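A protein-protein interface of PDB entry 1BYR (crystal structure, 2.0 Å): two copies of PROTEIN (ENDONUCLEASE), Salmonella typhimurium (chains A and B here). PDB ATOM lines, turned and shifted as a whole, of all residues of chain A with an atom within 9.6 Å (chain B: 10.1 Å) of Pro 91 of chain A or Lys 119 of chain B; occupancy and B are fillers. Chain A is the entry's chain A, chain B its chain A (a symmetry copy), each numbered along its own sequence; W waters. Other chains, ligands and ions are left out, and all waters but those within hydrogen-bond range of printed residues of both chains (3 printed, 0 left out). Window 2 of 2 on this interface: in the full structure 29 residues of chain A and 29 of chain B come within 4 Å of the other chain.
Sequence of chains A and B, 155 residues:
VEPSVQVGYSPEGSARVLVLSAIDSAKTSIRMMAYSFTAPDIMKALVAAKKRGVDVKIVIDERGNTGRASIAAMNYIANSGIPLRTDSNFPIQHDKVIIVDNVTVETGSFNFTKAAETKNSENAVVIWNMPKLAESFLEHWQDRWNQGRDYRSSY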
ATOM      1  N   TYR A  35      23.647  35.059 -17.483  1.00  0.00           N
ATOM      2  CA  TYR A  35      23.801  33.665 -17.878  1.00  0.00           C
ATOM      3  C   TYR A  35      24.995  33.861 -18.824  1.00  0.00           C
ATOM      4  O   TYR A  35      26.067  34.225 -18.367  1.00  0.00           O
ATOM      5  CB  TYR A  35      22.552  33.192 -18.620  1.00  0.00           C
ATOM      6  CG  TYR A  35      22.674  31.830 -19.267  1.00  0.00           C
ATOM      7  CD1 TYR A  35      23.393  30.807 -18.661  1.00  0.00           C
ATOM      8  CD2 TYR A  35      22.063  31.568 -20.483  1.00  0.00           C
ATOM      9  CE1 TYR A  35      23.502  29.554 -19.259  1.00  0.00           C
ATOM     10  CE2 TYR A  35      22.167  30.320 -21.091  1.00  0.00           C
ATOM     11  CZ  TYR A  35      22.883  29.314 -20.473  1.00  0.00           C
ATOM     12  OH  TYR A  35      22.970  28.073 -21.065  1.00  0.00           O
ATOM     13  N   ASP A  61      26.422  32.720 -14.348  1.00  0.00           N
ATOM     14  CA  ASP A  61      26.290  31.277 -14.396  1.00  0.00           C
ATOM     15  C   ASP A  61      27.651  30.670 -14.712  1.00  0.00           C
ATOM     16  O   ASP A  61      28.354  31.149 -15.611  1.00  0.00           O
ATOM     17  CB  ASP A  61      25.298  30.870 -15.492  1.00  0.00           C
ATOM     18  CG  ASP A  61      25.132  29.382 -15.572  1.00  0.00           C
ATOM     19  OD1 ASP A  61      24.533  28.815 -14.642  1.00  0.00           O
ATOM     20  OD2 ASP A  61      25.605  28.789 -16.558  1.00  0.00           O
ATOM     21  N   GLU A  62      28.009  29.610 -13.996  1.00  0.00           N
ATOM     22  CA  GLU A  62      29.303  28.963 -14.199  1.00  0.00           C
ATOM     23  C   GLU A  62      29.413  28.046 -15.407  1.00  0.00           C
ATOM     24  O   GLU A  62      30.280  28.244 -16.264  1.00  0.00           O
ATOM     25  CB  GLU A  62      29.694  28.180 -12.947  1.00  0.00           C
ATOM     26  CG  GLU A  62      31.136  27.721 -12.936  1.00  0.00           C
ATOM     27  CD  GLU A  62      31.537  27.110 -11.611  1.00  0.00           C
ATOM     28  OE1 GLU A  62      31.297  27.746 -10.554  1.00  0.00           O
ATOM     29  OE2 GLU A  62      32.087  25.988 -11.630  1.00  0.00           O
ATOM     30  N   ARG A  63      28.540  27.045 -15.496  1.00  0.00           N
ATOM     31  CA  ARG A  63      28.596  26.094 -16.612  1.00  0.00           C
ATOM     32  C   ARG A  63      28.463  26.676 -18.004  1.00  0.00           C
ATOM     33  O   ARG A  63      29.056  26.158 -18.949  1.00  0.00           O
ATOM     34  CB  ARG A  63      27.536  25.010 -16.437  1.00  0.00           C
ATOM     35  CG  ARG A  63      27.633  24.230 -15.147  1.00  0.00           C
ATOM     36  CD  ARG A  63      26.614  23.098 -15.190  1.00  0.00           C
ATOM     37  NE  ARG A  63      26.301  22.740 -16.570  1.00  0.00           N
ATOM     38  CZ  ARG A  63      25.085  22.763 -17.102  1.00  0.00           C
ATOM     39  NH1 ARG A  63      24.048  23.125 -16.371  1.00  0.00           N
ATOM     40  NH2 ARG A  63      24.911  22.420 -18.371  1.00  0.00           N
ATOM     41  N   GLY A  64      27.673  27.737 -18.128  1.00  0.00           N
ATOM     42  CA  GLY A  64      27.470  28.357 -19.421  1.00  0.00           C
ATOM     43  C   GLY A  64      28.478  29.437 -19.773  1.00  0.00           C
ATOM     44  O   GLY A  64      28.299  30.157 -20.747  1.00  0.00           O
ATOM     45  N   ASN A  65      29.534  29.563 -18.977  1.00  0.00           N
ATOM     46  CA  ASN A  65      30.559  30.575 -19.235  1.00  0.00           C
ATOM     47  C   ASN A  65      31.997  30.020 -19.279  1.00  0.00           C
ATOM     48  O   ASN A  65      32.915  30.542 -18.626  1.00  0.00           O
ATOM     49  CB  ASN A  65      30.447  31.694 -18.199  1.00  0.00           C
ATOM     50  CG  ASN A  65      29.375  32.697 -18.555  1.00  0.00           C
ATOM     51  OD1 ASN A  65      29.374  33.259 -19.648  1.00  0.00           O
ATOM     52  ND2 ASN A  65      28.440  32.924 -17.643  1.00  0.00           N
ATOM     53  N   ASP A  87      28.561  31.101 -10.482  1.00  0.00           N
ATOM     54  CA  ASP A  87      27.642  30.372  -9.606  1.00  0.00           C
ATOM     55  C   ASP A  87      27.195  29.102 -10.305  1.00  0.00           C
ATOM     56  O   ASP A  87      26.688  29.145 -11.427  1.00  0.00           O
ATOM     57  CB  ASP A  87      26.440  31.275  -9.292  1.00  0.00           C
ATOM     58  CG  ASP A  87      25.343  30.570  -8.500  1.00  0.00           C
ATOM     59  OD1 ASP A  87      25.580  29.489  -7.934  1.00  0.00           O
ATOM     60  OD2 ASP A  87      24.226  31.126  -8.439  1.00  0.00           O
ATOM     61  N   SER A  88      27.408  27.963  -9.652  1.00  0.00           N
ATOM     62  CA  SER A  88      27.035  26.679 -10.225  1.00  0.00           C
ATOM     63  C   SER A  88      26.032  25.931  -9.365  1.00  0.00           C
ATOM     64  O   SER A  88      25.787  24.754  -9.582  1.00  0.00           O
ATOM     65  CB  SER A  88      28.283  25.806 -10.379  1.00  0.00           C
ATOM     66  OG  SER A  88      28.869  25.554  -9.109  1.00  0.00           O
ATOM     67  N   ASN A  89      25.466  26.611  -8.381  1.00  0.00           N
ATOM     68  CA  ASN A  89      24.514  25.970  -7.492  1.00  0.00           C
ATOM     69  C   ASN A  89      23.141  25.717  -8.103  1.00  0.00           C
ATOM     70  O   ASN A  89      22.278  25.114  -7.473  1.00  0.00           O
ATOM     71  CB  ASN A  89      24.393  26.774  -6.202  1.00  0.00           C
ATOM     72  CG  ASN A  89      25.573  26.534  -5.272  1.00  0.00           C
ATOM     73  OD1 ASN A  89      26.236  25.487  -5.346  1.00  0.00           O
ATOM     74  ND2 ASN A  89      25.854  27.490  -4.400  1.00  0.00           N
ATOM     75  N   PHE A  90      22.963  26.159  -9.342  1.00  0.00           N
ATOM     76  CA  PHE A  90      21.706  25.980 -10.052  1.00  0.00           C
ATOM     77  C   PHE A  90      21.981  25.327 -11.411  1.00  0.00           C
ATOM     78  O   PHE A  90      23.010  25.605 -12.040  1.00  0.00           O
ATOM     79  CB  PHE A  90      21.018  27.341 -10.265  1.00  0.00           C
ATOM     80  CG  PHE A  90      20.708  28.093  -8.984  1.00  0.00           C
ATOM     81  CD1 PHE A  90      21.639  28.968  -8.426  1.00  0.00           C
ATOM     82  CD2 PHE A  90      19.477  27.948  -8.357  1.00  0.00           C
ATOM     83  CE1 PHE A  90      21.352  29.682  -7.273  1.00  0.00           C
ATOM     84  CE2 PHE A  90      19.189  28.661  -7.202  1.00  0.00           C
ATOM     85  CZ  PHE A  90      20.136  29.535  -6.661  1.00  0.00           C
ATOM     86  N   PRO A  91      21.100  24.412 -11.869  1.00  0.00           N
ATOM     87  CA  PRO A  91      21.419  23.841 -13.179  1.00  0.00           C
ATOM     88  C   PRO A  91      21.788  24.987 -14.128  1.00  0.00           C
ATOM     89  O   PRO A  91      22.710  24.868 -14.936  1.00  0.00           O
ATOM     90  CB  PRO A  91      20.131  23.111 -13.571  1.00  0.00           C
ATOM     91  CG  PRO A  91      19.558  22.687 -12.266  1.00  0.00           C
ATOM     92  CD  PRO A  91      19.884  23.813 -11.293  1.00  0.00           C
ATOM     93  N   ILE A  92      21.050  26.090 -14.030  1.00  0.00           N
ATOM     94  CA  ILE A  92      21.324  27.292 -14.827  1.00  0.00           C
ATOM     95  C   ILE A  92      20.960  28.566 -14.048  1.00  0.00           C
ATOM     96  O   ILE A  92      19.829  28.696 -13.580  1.00  0.00           O
ATOM     97  CB  ILE A  92      20.501  27.342 -16.159  1.00  0.00           C
ATOM     98  CG1 ILE A  92      20.706  26.071 -16.988  1.00  0.00           C
ATOM     99  CG2 ILE A  92      20.935  28.564 -16.992  1.00  0.00           C
ATOM    100  CD1 ILE A  92      20.094  26.176 -18.362  1.00  0.00           C
ATOM    101  N   GLN A  93      21.923  29.476 -13.849  1.00  0.00           N
ATOM    102  CA  GLN A  93      21.623  30.761 -13.208  1.00  0.00           C
ATOM    103  C   GLN A  93      21.228  31.541 -14.449  1.00  0.00           C
ATOM    104  O   GLN A  93      22.059  32.182 -15.098  1.00  0.00           O
ATOM    105  CB  GLN A  93      22.855  31.405 -12.562  1.00  0.00           C
ATOM    106  CG  GLN A  93      22.494  32.376 -11.449  1.00  0.00           C
ATOM    107  CD  GLN A  93      23.583  33.397 -11.169  1.00  0.00           C
ATOM    108  OE1 GLN A  93      23.759  34.355 -11.901  1.00  0.00           O
ATOM    109  NE2 GLN A  93      24.311  33.178 -10.102  1.00  0.00           N
ATOM    110  N   HIS A  94      19.949  31.455 -14.785  1.00  0.00           N
ATOM    111  CA  HIS A  94      19.396  32.051 -16.004  1.00  0.00           C
ATOM    112  C   HIS A  94      19.035  33.542 -16.058  1.00  0.00           C
ATOM    113  O   HIS A  94      18.717  34.053 -17.137  1.00  0.00           O
ATOM    114  CB  HIS A  94      18.180  31.204 -16.427  1.00  0.00           C
ATOM    115  CG  HIS A  94      17.846  31.277 -17.884  1.00  0.00           C
ATOM    116  ND1 HIS A  94      16.659  31.785 -18.348  1.00  0.00           N
ATOM    117  CD2 HIS A  94      18.565  30.927 -18.981  1.00  0.00           C
ATOM    118  CE1 HIS A  94      16.635  31.728 -19.672  1.00  0.00           C
ATOM    119  NE2 HIS A  94      17.786  31.218 -20.077  1.00  0.00           N
ATOM    120  N   ASP A  95      19.091  34.241 -14.922  1.00  0.00           N
ATOM    121  CA  ASP A  95      18.758  35.667 -14.875  1.00  0.00           C
ATOM    122  C   ASP A  95      19.652  36.548 -15.740  1.00  0.00           C
ATOM    123  O   ASP A  95      20.858  36.319 -15.840  1.00  0.00           O
ATOM    124  CB  ASP A  95      18.854  36.211 -13.442  1.00  0.00           C
ATOM    125  CG  ASP A  95      18.048  35.401 -12.451  1.00  0.00           C
ATOM    126  OD1 ASP A  95      18.604  34.430 -11.895  1.00  0.00           O
ATOM    127  OD2 ASP A  95      16.863  35.732 -12.222  1.00  0.00           O
ATOM    128  N   ARG A 144      22.337  34.697  -4.747  1.00  0.00           N
ATOM    129  CA  ARG A 144      23.113  34.016  -5.780  1.00  0.00           C
ATOM    130  C   ARG A 144      24.594  34.347  -5.642  1.00  0.00           C
ATOM    131  O   ARG A 144      25.439  33.482  -5.800  1.00  0.00           O
ATOM    132  CB  ARG A 144      22.614  34.431  -7.164  1.00  0.00           C
ATOM    133  CG  ARG A 144      21.390  33.627  -7.693  1.00  0.00           C
ATOM    134  CD  ARG A 144      20.335  33.330  -6.620  1.00  0.00           C
ATOM    135  NE  ARG A 144      19.103  32.787  -7.209  1.00  0.00           N
ATOM    136  CZ  ARG A 144      18.015  32.445  -6.518  1.00  0.00           C
ATOM    137  NH1 ARG A 144      17.989  32.575  -5.199  1.00  0.00           N
ATOM    138  NH2 ARG A 144      16.932  32.008  -7.157  1.00  0.00           N
ATOM    139  N   GLN A 147      26.672  32.432  -2.877  1.00  0.00           N
ATOM    140  CA  GLN A 147      27.090  31.053  -3.084  1.00  0.00           C
ATOM    141  C   GLN A 147      27.919  30.915  -4.351  1.00  0.00           C
ATOM    142  O   GLN A 147      28.003  29.830  -4.948  1.00  0.00           O
ATOM    143  CB  GLN A 147      25.880  30.122  -3.150  1.00  0.00           C
ATOM    144  CG  GLN A 147      24.852  30.500  -4.163  1.00  0.00           C
ATOM    145  CD  GLN A 147      23.532  29.855  -3.860  1.00  0.00           C
ATOM    146  OE1 GLN A 147      23.436  28.635  -3.706  1.00  0.00           O
ATOM    147  NE2 GLN A 147      22.496  30.659  -3.767  1.00  0.00           N
ATOM    148  N   TYR B   9      10.464  34.714  -8.334  1.00  0.00           N
ATOM    149  CA  TYR B   9      11.714  34.068  -8.720  1.00  0.00           C
ATOM    150  C   TYR B   9      11.634  32.550  -8.716  1.00  0.00           C
ATOM    151  O   TYR B   9      10.756  31.961  -8.091  1.00  0.00           O
ATOM    152  CB  TYR B   9      12.831  34.502  -7.761  1.00  0.00           C
ATOM    153  CG  TYR B   9      12.899  35.999  -7.528  1.00  0.00           C
ATOM    154  CD1 TYR B   9      13.408  36.846  -8.508  1.00  0.00           C
ATOM    155  CD2 TYR B   9      12.453  36.568  -6.326  1.00  0.00           C
ATOM    156  CE1 TYR B   9      13.475  38.222  -8.307  1.00  0.00           C
ATOM    157  CE2 TYR B   9      12.517  37.951  -6.120  1.00  0.00           C
ATOM    158  CZ  TYR B   9      13.028  38.766  -7.112  1.00  0.00           C
ATOM    159  OH  TYR B   9      13.076  40.132  -6.929  1.00  0.00           O
ATOM    160  N   SER B  10      12.561  31.924  -9.441  1.00  0.00           N
ATOM    161  CA  SER B  10      12.679  30.478  -9.489  1.00  0.00           C
ATOM    162  C   SER B  10      14.092  30.206  -8.982  1.00  0.00           C
ATOM    163  O   SER B  10      14.974  31.053  -9.127  1.00  0.00           O
ATOM    164  CB  SER B  10      12.508  29.953 -10.918  1.00  0.00           C
ATOM    165  OG  SER B  10      11.190  30.139 -11.388  1.00  0.00           O
ATOM    166  N   PRO B  11      14.337  29.035  -8.369  1.00  0.00           N
ATOM    167  CA  PRO B  11      13.397  27.953  -8.088  1.00  0.00           C
ATOM    168  C   PRO B  11      12.515  28.172  -6.848  1.00  0.00           C
ATOM    169  O   PRO B  11      11.833  27.252  -6.407  1.00  0.00           O
ATOM    170  CB  PRO B  11      14.313  26.746  -7.919  1.00  0.00           C
ATOM    171  CG  PRO B  11      15.529  27.325  -7.275  1.00  0.00           C
ATOM    172  CD  PRO B  11      15.693  28.710  -7.890  1.00  0.00           C
ATOM    173  N   GLU B  12      12.524  29.379  -6.294  1.00  0.00           N
ATOM    174  CA  GLU B  12      11.721  29.692  -5.106  1.00  0.00           C
ATOM    175  C   GLU B  12      10.245  29.284  -5.254  1.00  0.00           C
ATOM    176  O   GLU B  12       9.619  28.770  -4.318  1.00  0.00           O
ATOM    177  CB  GLU B  12      11.807  31.186  -4.799  1.00  0.00           C
ATOM    178  CG  GLU B  12      13.030  31.596  -3.944  1.00  0.00           C
ATOM    179  CD  GLU B  12      14.328  31.726  -4.748  1.00  0.00           C
ATOM    180  OE1 GLU B  12      14.363  31.357  -5.941  1.00  0.00           O
ATOM    181  OE2 GLU B  12      15.324  32.203  -4.173  1.00  0.00           O
ATOM    182  N   GLY B  13       9.683  29.540  -6.428  1.00  0.00           N
ATOM    183  CA  GLY B  13       8.290  29.205  -6.658  1.00  0.00           C
ATOM    184  C   GLY B  13       7.422  30.413  -6.941  1.00  0.00           C
ATOM    185  O   GLY B  13       6.369  30.301  -7.562  1.00  0.00           O
ATOM    186  N   ALA B  15       7.911  32.925  -9.014  1.00  0.00           N
ATOM    187  CA  ALA B  15       7.834  33.307 -10.426  1.00  0.00           C
ATOM    188  C   ALA B  15       6.690  32.550 -11.110  1.00  0.00           C
ATOM    189  O   ALA B  15       5.838  33.136 -11.784  1.00  0.00           O
ATOM    190  CB  ALA B  15       9.136  32.997 -11.132  1.00  0.00           C
ATOM    191  N   ARG B  16       6.679  31.239 -10.936  1.00  0.00           N
ATOM    192  CA  ARG B  16       5.653  30.411 -11.537  1.00  0.00           C
ATOM    193  C   ARG B  16       4.257  30.909 -11.134  1.00  0.00           C
ATOM    194  O   ARG B  16       3.396  31.129 -11.986  1.00  0.00           O
ATOM    195  CB  ARG B  16       5.868  28.955 -11.107  1.00  0.00           C
ATOM    196  CG  ARG B  16       4.736  28.005 -11.439  1.00  0.00           C
ATOM    197  CD  ARG B  16       4.705  26.860 -10.437  1.00  0.00           C
ATOM    198  NE  ARG B  16       4.777  25.575 -11.116  1.00  0.00           N
ATOM    199  CZ  ARG B  16       5.514  24.545 -10.720  1.00  0.00           C
ATOM    200  NH1 ARG B  16       6.275  24.644  -9.645  1.00  0.00           N
ATOM    201  NH2 ARG B  16       5.499  23.418 -11.415  1.00  0.00           N
ATOM    202  N   PHE B 110      12.336  34.036 -17.224  1.00  0.00           N
ATOM    203  CA  PHE B 110      11.473  32.854 -17.117  1.00  0.00           C
ATOM    204  C   PHE B 110      10.894  32.255 -18.415  1.00  0.00           C
ATOM    205  O   PHE B 110      10.035  32.868 -19.069  1.00  0.00           O
ATOM    206  CB  PHE B 110      10.341  33.194 -16.124  1.00  0.00           C
ATOM    207  CG  PHE B 110       9.405  32.041 -15.797  1.00  0.00           C
ATOM    208  CD1 PHE B 110       8.273  31.796 -16.572  1.00  0.00           C
ATOM    209  CD2 PHE B 110       9.590  31.282 -14.654  1.00  0.00           C
ATOM    210  CE1 PHE B 110       7.347  30.813 -16.198  1.00  0.00           C
ATOM    211  CE2 PHE B 110       8.658  30.294 -14.281  1.00  0.00           C
ATOM    212  CZ  PHE B 110       7.547  30.068 -15.047  1.00  0.00           C
ATOM    213  N   ASN B 111      11.369  31.065 -18.792  1.00  0.00           N
ATOM    214  CA  ASN B 111      10.841  30.381 -19.982  1.00  0.00           C
ATOM    215  C   ASN B 111       9.644  29.593 -19.490  1.00  0.00           C
ATOM    216  O   ASN B 111       9.563  29.240 -18.315  1.00  0.00           O
ATOM    217  CB  ASN B 111      11.837  29.392 -20.580  1.00  0.00           C
ATOM    218  CG  ASN B 111      12.851  30.051 -21.458  1.00  0.00           C
ATOM    219  OD1 ASN B 111      14.024  30.152 -21.102  1.00  0.00           O
ATOM    220  ND2 ASN B 111      12.425  30.513 -22.608  1.00  0.00           N
ATOM    221  N   THR B 113       8.624  26.660 -19.114  1.00  0.00           N
ATOM    222  CA  THR B 113       9.034  25.281 -18.968  1.00  0.00           C
ATOM    223  C   THR B 113       9.096  24.886 -17.518  1.00  0.00           C
ATOM    224  O   THR B 113       9.096  25.719 -16.611  1.00  0.00           O
ATOM    225  CB  THR B 113      10.452  25.051 -19.514  1.00  0.00           C
ATOM    226  OG1 THR B 113      11.393  25.720 -18.653  1.00  0.00           O
ATOM    227  CG2 THR B 113      10.578  25.589 -20.924  1.00  0.00           C
ATOM    228  N   LYS B 114       9.183  23.577 -17.339  1.00  0.00           N
ATOM    229  CA  LYS B 114       9.292  22.940 -16.029  1.00  0.00           C
ATOM    230  C   LYS B 114      10.642  23.348 -15.361  1.00  0.00           C
ATOM    231  O   LYS B 114      10.692  23.751 -14.178  1.00  0.00           O
ATOM    232  CB  LYS B 114       9.214  21.406 -16.213  1.00  0.00           C
ATOM    233  CG  LYS B 114       8.474  20.924 -17.520  1.00  0.00           C
ATOM    234  CD  LYS B 114       9.147  21.373 -18.866  1.00  0.00           C
ATOM    235  CE  LYS B 114      10.519  20.754 -19.159  1.00  0.00           C
ATOM    236  NZ  LYS B 114      11.668  21.639 -18.752  1.00  0.00           N
ATOM    237  N   ALA B 115      11.729  23.264 -16.127  1.00  0.00           N
ATOM    238  CA  ALA B 115      13.046  23.625 -15.608  1.00  0.00           C
ATOM    239  C   ALA B 115      13.031  25.074 -15.117  1.00  0.00           C
ATOM    240  O   ALA B 115      13.622  25.394 -14.090  1.00  0.00           O
ATOM    241  CB  ALA B 115      14.101  23.430 -16.682  1.00  0.00           C
ATOM    242  N   ALA B 116      12.331  25.944 -15.840  1.00  0.00           N
ATOM    243  CA  ALA B 116      12.234  27.355 -15.461  1.00  0.00           C
ATOM    244  C   ALA B 116      11.465  27.580 -14.153  1.00  0.00           C
ATOM    245  O   ALA B 116      11.736  28.528 -13.402  1.00  0.00           O
ATOM    246  CB  ALA B 116      11.559  28.135 -16.576  1.00  0.00           C
ATOM    247  N   GLU B 117      10.494  26.709 -13.898  1.00  0.00           N
ATOM    248  CA  GLU B 117       9.652  26.797 -12.705  1.00  0.00           C
ATOM    249  C   GLU B 117      10.242  26.204 -11.438  1.00  0.00           C
ATOM    250  O   GLU B 117      10.062  26.735 -10.342  1.00  0.00           O
ATOM    251  CB  GLU B 117       8.314  26.074 -12.946  1.00  0.00           C
ATOM    252  CG  GLU B 117       7.592  26.464 -14.232  1.00  0.00           C
ATOM    253  CD  GLU B 117       6.250  25.741 -14.432  1.00  0.00           C
ATOM    254  OE1 GLU B 117       6.191  24.506 -14.248  1.00  0.00           O
ATOM    255  OE2 GLU B 117       5.258  26.416 -14.783  1.00  0.00           O
ATOM    256  N   THR B 118      10.982  25.124 -11.621  1.00  0.00           N
ATOM    257  CA  THR B 118      11.484  24.352 -10.497  1.00  0.00           C
ATOM    258  C   THR B 118      12.991  24.132 -10.298  1.00  0.00           C
ATOM    259  O   THR B 118      13.414  23.699  -9.228  1.00  0.00           O
ATOM    260  CB  THR B 118      10.771  22.970 -10.575  1.00  0.00           C
ATOM    261  OG1 THR B 118       9.615  22.971  -9.730  1.00  0.00           O
ATOM    262  CG2 THR B 118      11.709  21.851 -10.251  1.00  0.00           C
ATOM    263  N   LYS B 119      13.799  24.437 -11.303  1.00  0.00           N
ATOM    264  CA  LYS B 119      15.243  24.178 -11.185  1.00  0.00           C
ATOM    265  C   LYS B 119      16.186  25.375 -11.341  1.00  0.00           C
ATOM    266  O   LYS B 119      17.102  25.553 -10.548  1.00  0.00           O
ATOM    267  CB  LYS B 119      15.659  23.106 -12.206  1.00  0.00           C
ATOM    268  CG  LYS B 119      14.690  21.928 -12.347  1.00  0.00           C
ATOM    269  CD  LYS B 119      15.138  20.736 -11.515  1.00  0.00           C
ATOM    270  CE  LYS B 119      14.027  19.681 -11.378  1.00  0.00           C
ATOM    271  NZ  LYS B 119      13.565  19.147 -12.704  1.00  0.00           N
ATOM    272  N   ASN B 120      15.968  26.168 -12.386  1.00  0.00           N
ATOM    273  CA  ASN B 120      16.819  27.316 -12.667  1.00  0.00           C
ATOM    274  C   ASN B 120      16.565  28.521 -11.785  1.00  0.00           C
ATOM    275  O   ASN B 120      15.522  28.634 -11.140  1.00  0.00           O
ATOM    276  CB  ASN B 120      16.611  27.754 -14.109  1.00  0.00           C
ATOM    277  CG  ASN B 120      16.978  26.675 -15.101  1.00  0.00           C
ATOM    278  OD1 ASN B 120      17.709  25.743 -14.787  1.00  0.00           O
ATOM    279  ND2 ASN B 120      16.462  26.796 -16.311  1.00  0.00           N
ATOM    280  N   SER B 121      17.545  29.417 -11.745  1.00  0.00           N
ATOM    281  CA  SER B 121      17.347  30.669 -11.039  1.00  0.00           C
ATOM    282  C   SER B 121      16.768  31.534 -12.157  1.00  0.00           C
ATOM    283  O   SER B 121      17.311  31.585 -13.281  1.00  0.00           O
ATOM    284  CB  SER B 121      18.664  31.267 -10.540  1.00  0.00           C
ATOM    285  OG  SER B 121      18.412  32.518  -9.929  1.00  0.00           O
ATOM    286  N   GLU B 122      15.628  32.163 -11.880  1.00  0.00           N
ATOM    287  CA  GLU B 122      14.944  33.006 -12.855  1.00  0.00           C
ATOM    288  C   GLU B 122      14.233  34.121 -12.135  1.00  0.00           C
ATOM    289  O   GLU B 122      14.104  34.119 -10.918  1.00  0.00           O
ATOM    290  CB  GLU B 122      13.842  32.240 -13.620  1.00  0.00           C
ATOM    291  CG  GLU B 122      14.185  30.863 -14.109  1.00  0.00           C
ATOM    292  CD  GLU B 122      14.733  30.865 -15.509  1.00  0.00           C
ATOM    293  OE1 GLU B 122      14.982  31.958 -16.050  1.00  0.00           O
ATOM    294  OE2 GLU B 122      14.913  29.767 -16.066  1.00  0.00           O
HETATM  295  O   HOH W   1      14.558  29.129 -18.387  1.00  0.00           O
HETATM  296  O   HOH W   2      16.386  30.932 -22.933  1.00  0.00           O
HETATM  297  O   HOH W   3      15.490  34.995  -4.974  1.00  0.00           O
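Among the printed residues, merely in contact across the chains: Pro 91 of chain A with Lys 119 of chain B (3.4 Å), His 94 of chain A with Asn 111 of chain B (3.4 Å), Phe 90 of chain A with Pro 11 of chain B (3.6 Å), Arg 144 of chain A with Pro 11 of chain B (3.6 Å) and Pro 91 of chain A with Asn 120 of chain B (3.8 Å).
No position is printed for both chains.
Of the 17 printed residues of chain A, 6 touch a printed residue of chain B. Hydrophobic or aromatic side chains of chain A within 4 Å of the printed part of chain B: Phe 90, Pro 91, Ile 92 and His 94. Hydrophobic or aromatic side chains of chain B that line the printed part of chain A: Pro 11.
N of Tyr 35 of chain A lies within hydrogen-bond range of O of Asp 95 of chain A, 3.5 Å away. O of Pro 91 of chain A is in hydrogen-bond range of NH1 of Arg 63 of chain A (2.6 Å). The backbone carbonyl oxygen (O) of Ser 10 of chain B is in hydrogen-bond range of the backbone NH (N) of Glu 122 of chain B, 3.0 Å away. The backbone carbonyl oxygen (O) of Ala 115 of chain B lies within hydrogen-bond range of the backbone NH (N) of Asn 120 of chain B, 3.0 Å away. The side-chain amide nitrogen of Asn 120 of chain B lies close to the side-chain carboxylate of Glu 122 of chain B.
Water W1 lies within hydrogen-bond range of OE2 of Glu 122 of chain B (2.4 Å), OD1 of Asn 111 of chain B (3.0 Å) and ND1 of His 94 of chain A (3.4 Å). Water W3 lies within hydrogen-bond range of OE2 of Glu 12 of chain B and NH1 of Arg 144 of chain A. Water W2 bridges OD1 of Asn 111 of chain B (3.1 Å) and NE2 of His 94 of chain A (3.2 Å).
The backbone NH (N) of Ile 92 of chain A is in hydrogen-bond range of the side-chain amide oxygen (OD1) of Asn 120 of chain B (3.4 Å). The backbone carbonyl oxygen (O) of Ile 92 of chain A sits at hydrogen-bond distance from the backbone NH (N) of Ser 121 of chain B, 3.0 Å away. The backbone carbonyl oxygen of Ser 121 of chain B is in hydrogen-bond range of the backbone NH of His 94 of chain A. A ring nitrogen (ND1) of His 94 of chain A is in hydrogen-bond range of the side-chain carboxylate of Glu 122 of chain B (2.9 Å). The side-chain hydroxyl (OG) of Ser 121 of chain B sits at hydrogen-bond distance from the side-chain carboxylate (OD1) of Asp 95 of chain A, 2.7 Å away. O of Ser 10 of chain B sits at hydrogen-bond distance from NH2 of Arg 144 of chain A (2.9 Å). NH1 of Arg 144 of chain A lies within salt-bridge range of OE2 of Glu 12 of chain B (2.9 Å). The side-chain hydroxyl of Ser 121 of chain B lies within hydrogen-bond range of the guanidinium group of Arg 144 of chain A (2.8 Å). The side-chain carboxylate (OD2) of Asp 95 of chain A sits close to the backbone carbonyl oxygen (O) of Glu 122 of chain B (3.5 Å).
Of the printed residues of chain B, Phe 90 of chain A touches Pro 11 (3.6 Å). Of chain B, only Lys 119 (3.4 Å) and Asn 120 (3.8 Å) come within 4 Å of Pro 91 of chain A. Printed residues of chain B within 4 Å of Asp 95 of chain A: Ser 121 (2.7 Å) and Glu 122 (3.1 Å). Gln 147 of chain A touches none of the printed residues of chain B. Of the printed residues of chain A, Pro 11 of chain B touches Phe 90 (3.6 Å) and Arg 144 (3.6 Å). Ala 15 of chain B touches none of the printed residues of chain A. No residue of chain A comes within 4 Å of Ala 115 of chain B. No residue of chain A comes within 4 Å of Thr 118 of chain B. Of chain A, only Pro 91 comes within 4 Å of Lys 119 of chain B. The nearest printed residue of chain A that does not touch Pro 11 of chain B is Pro 91 of chain A (6.9 Å).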
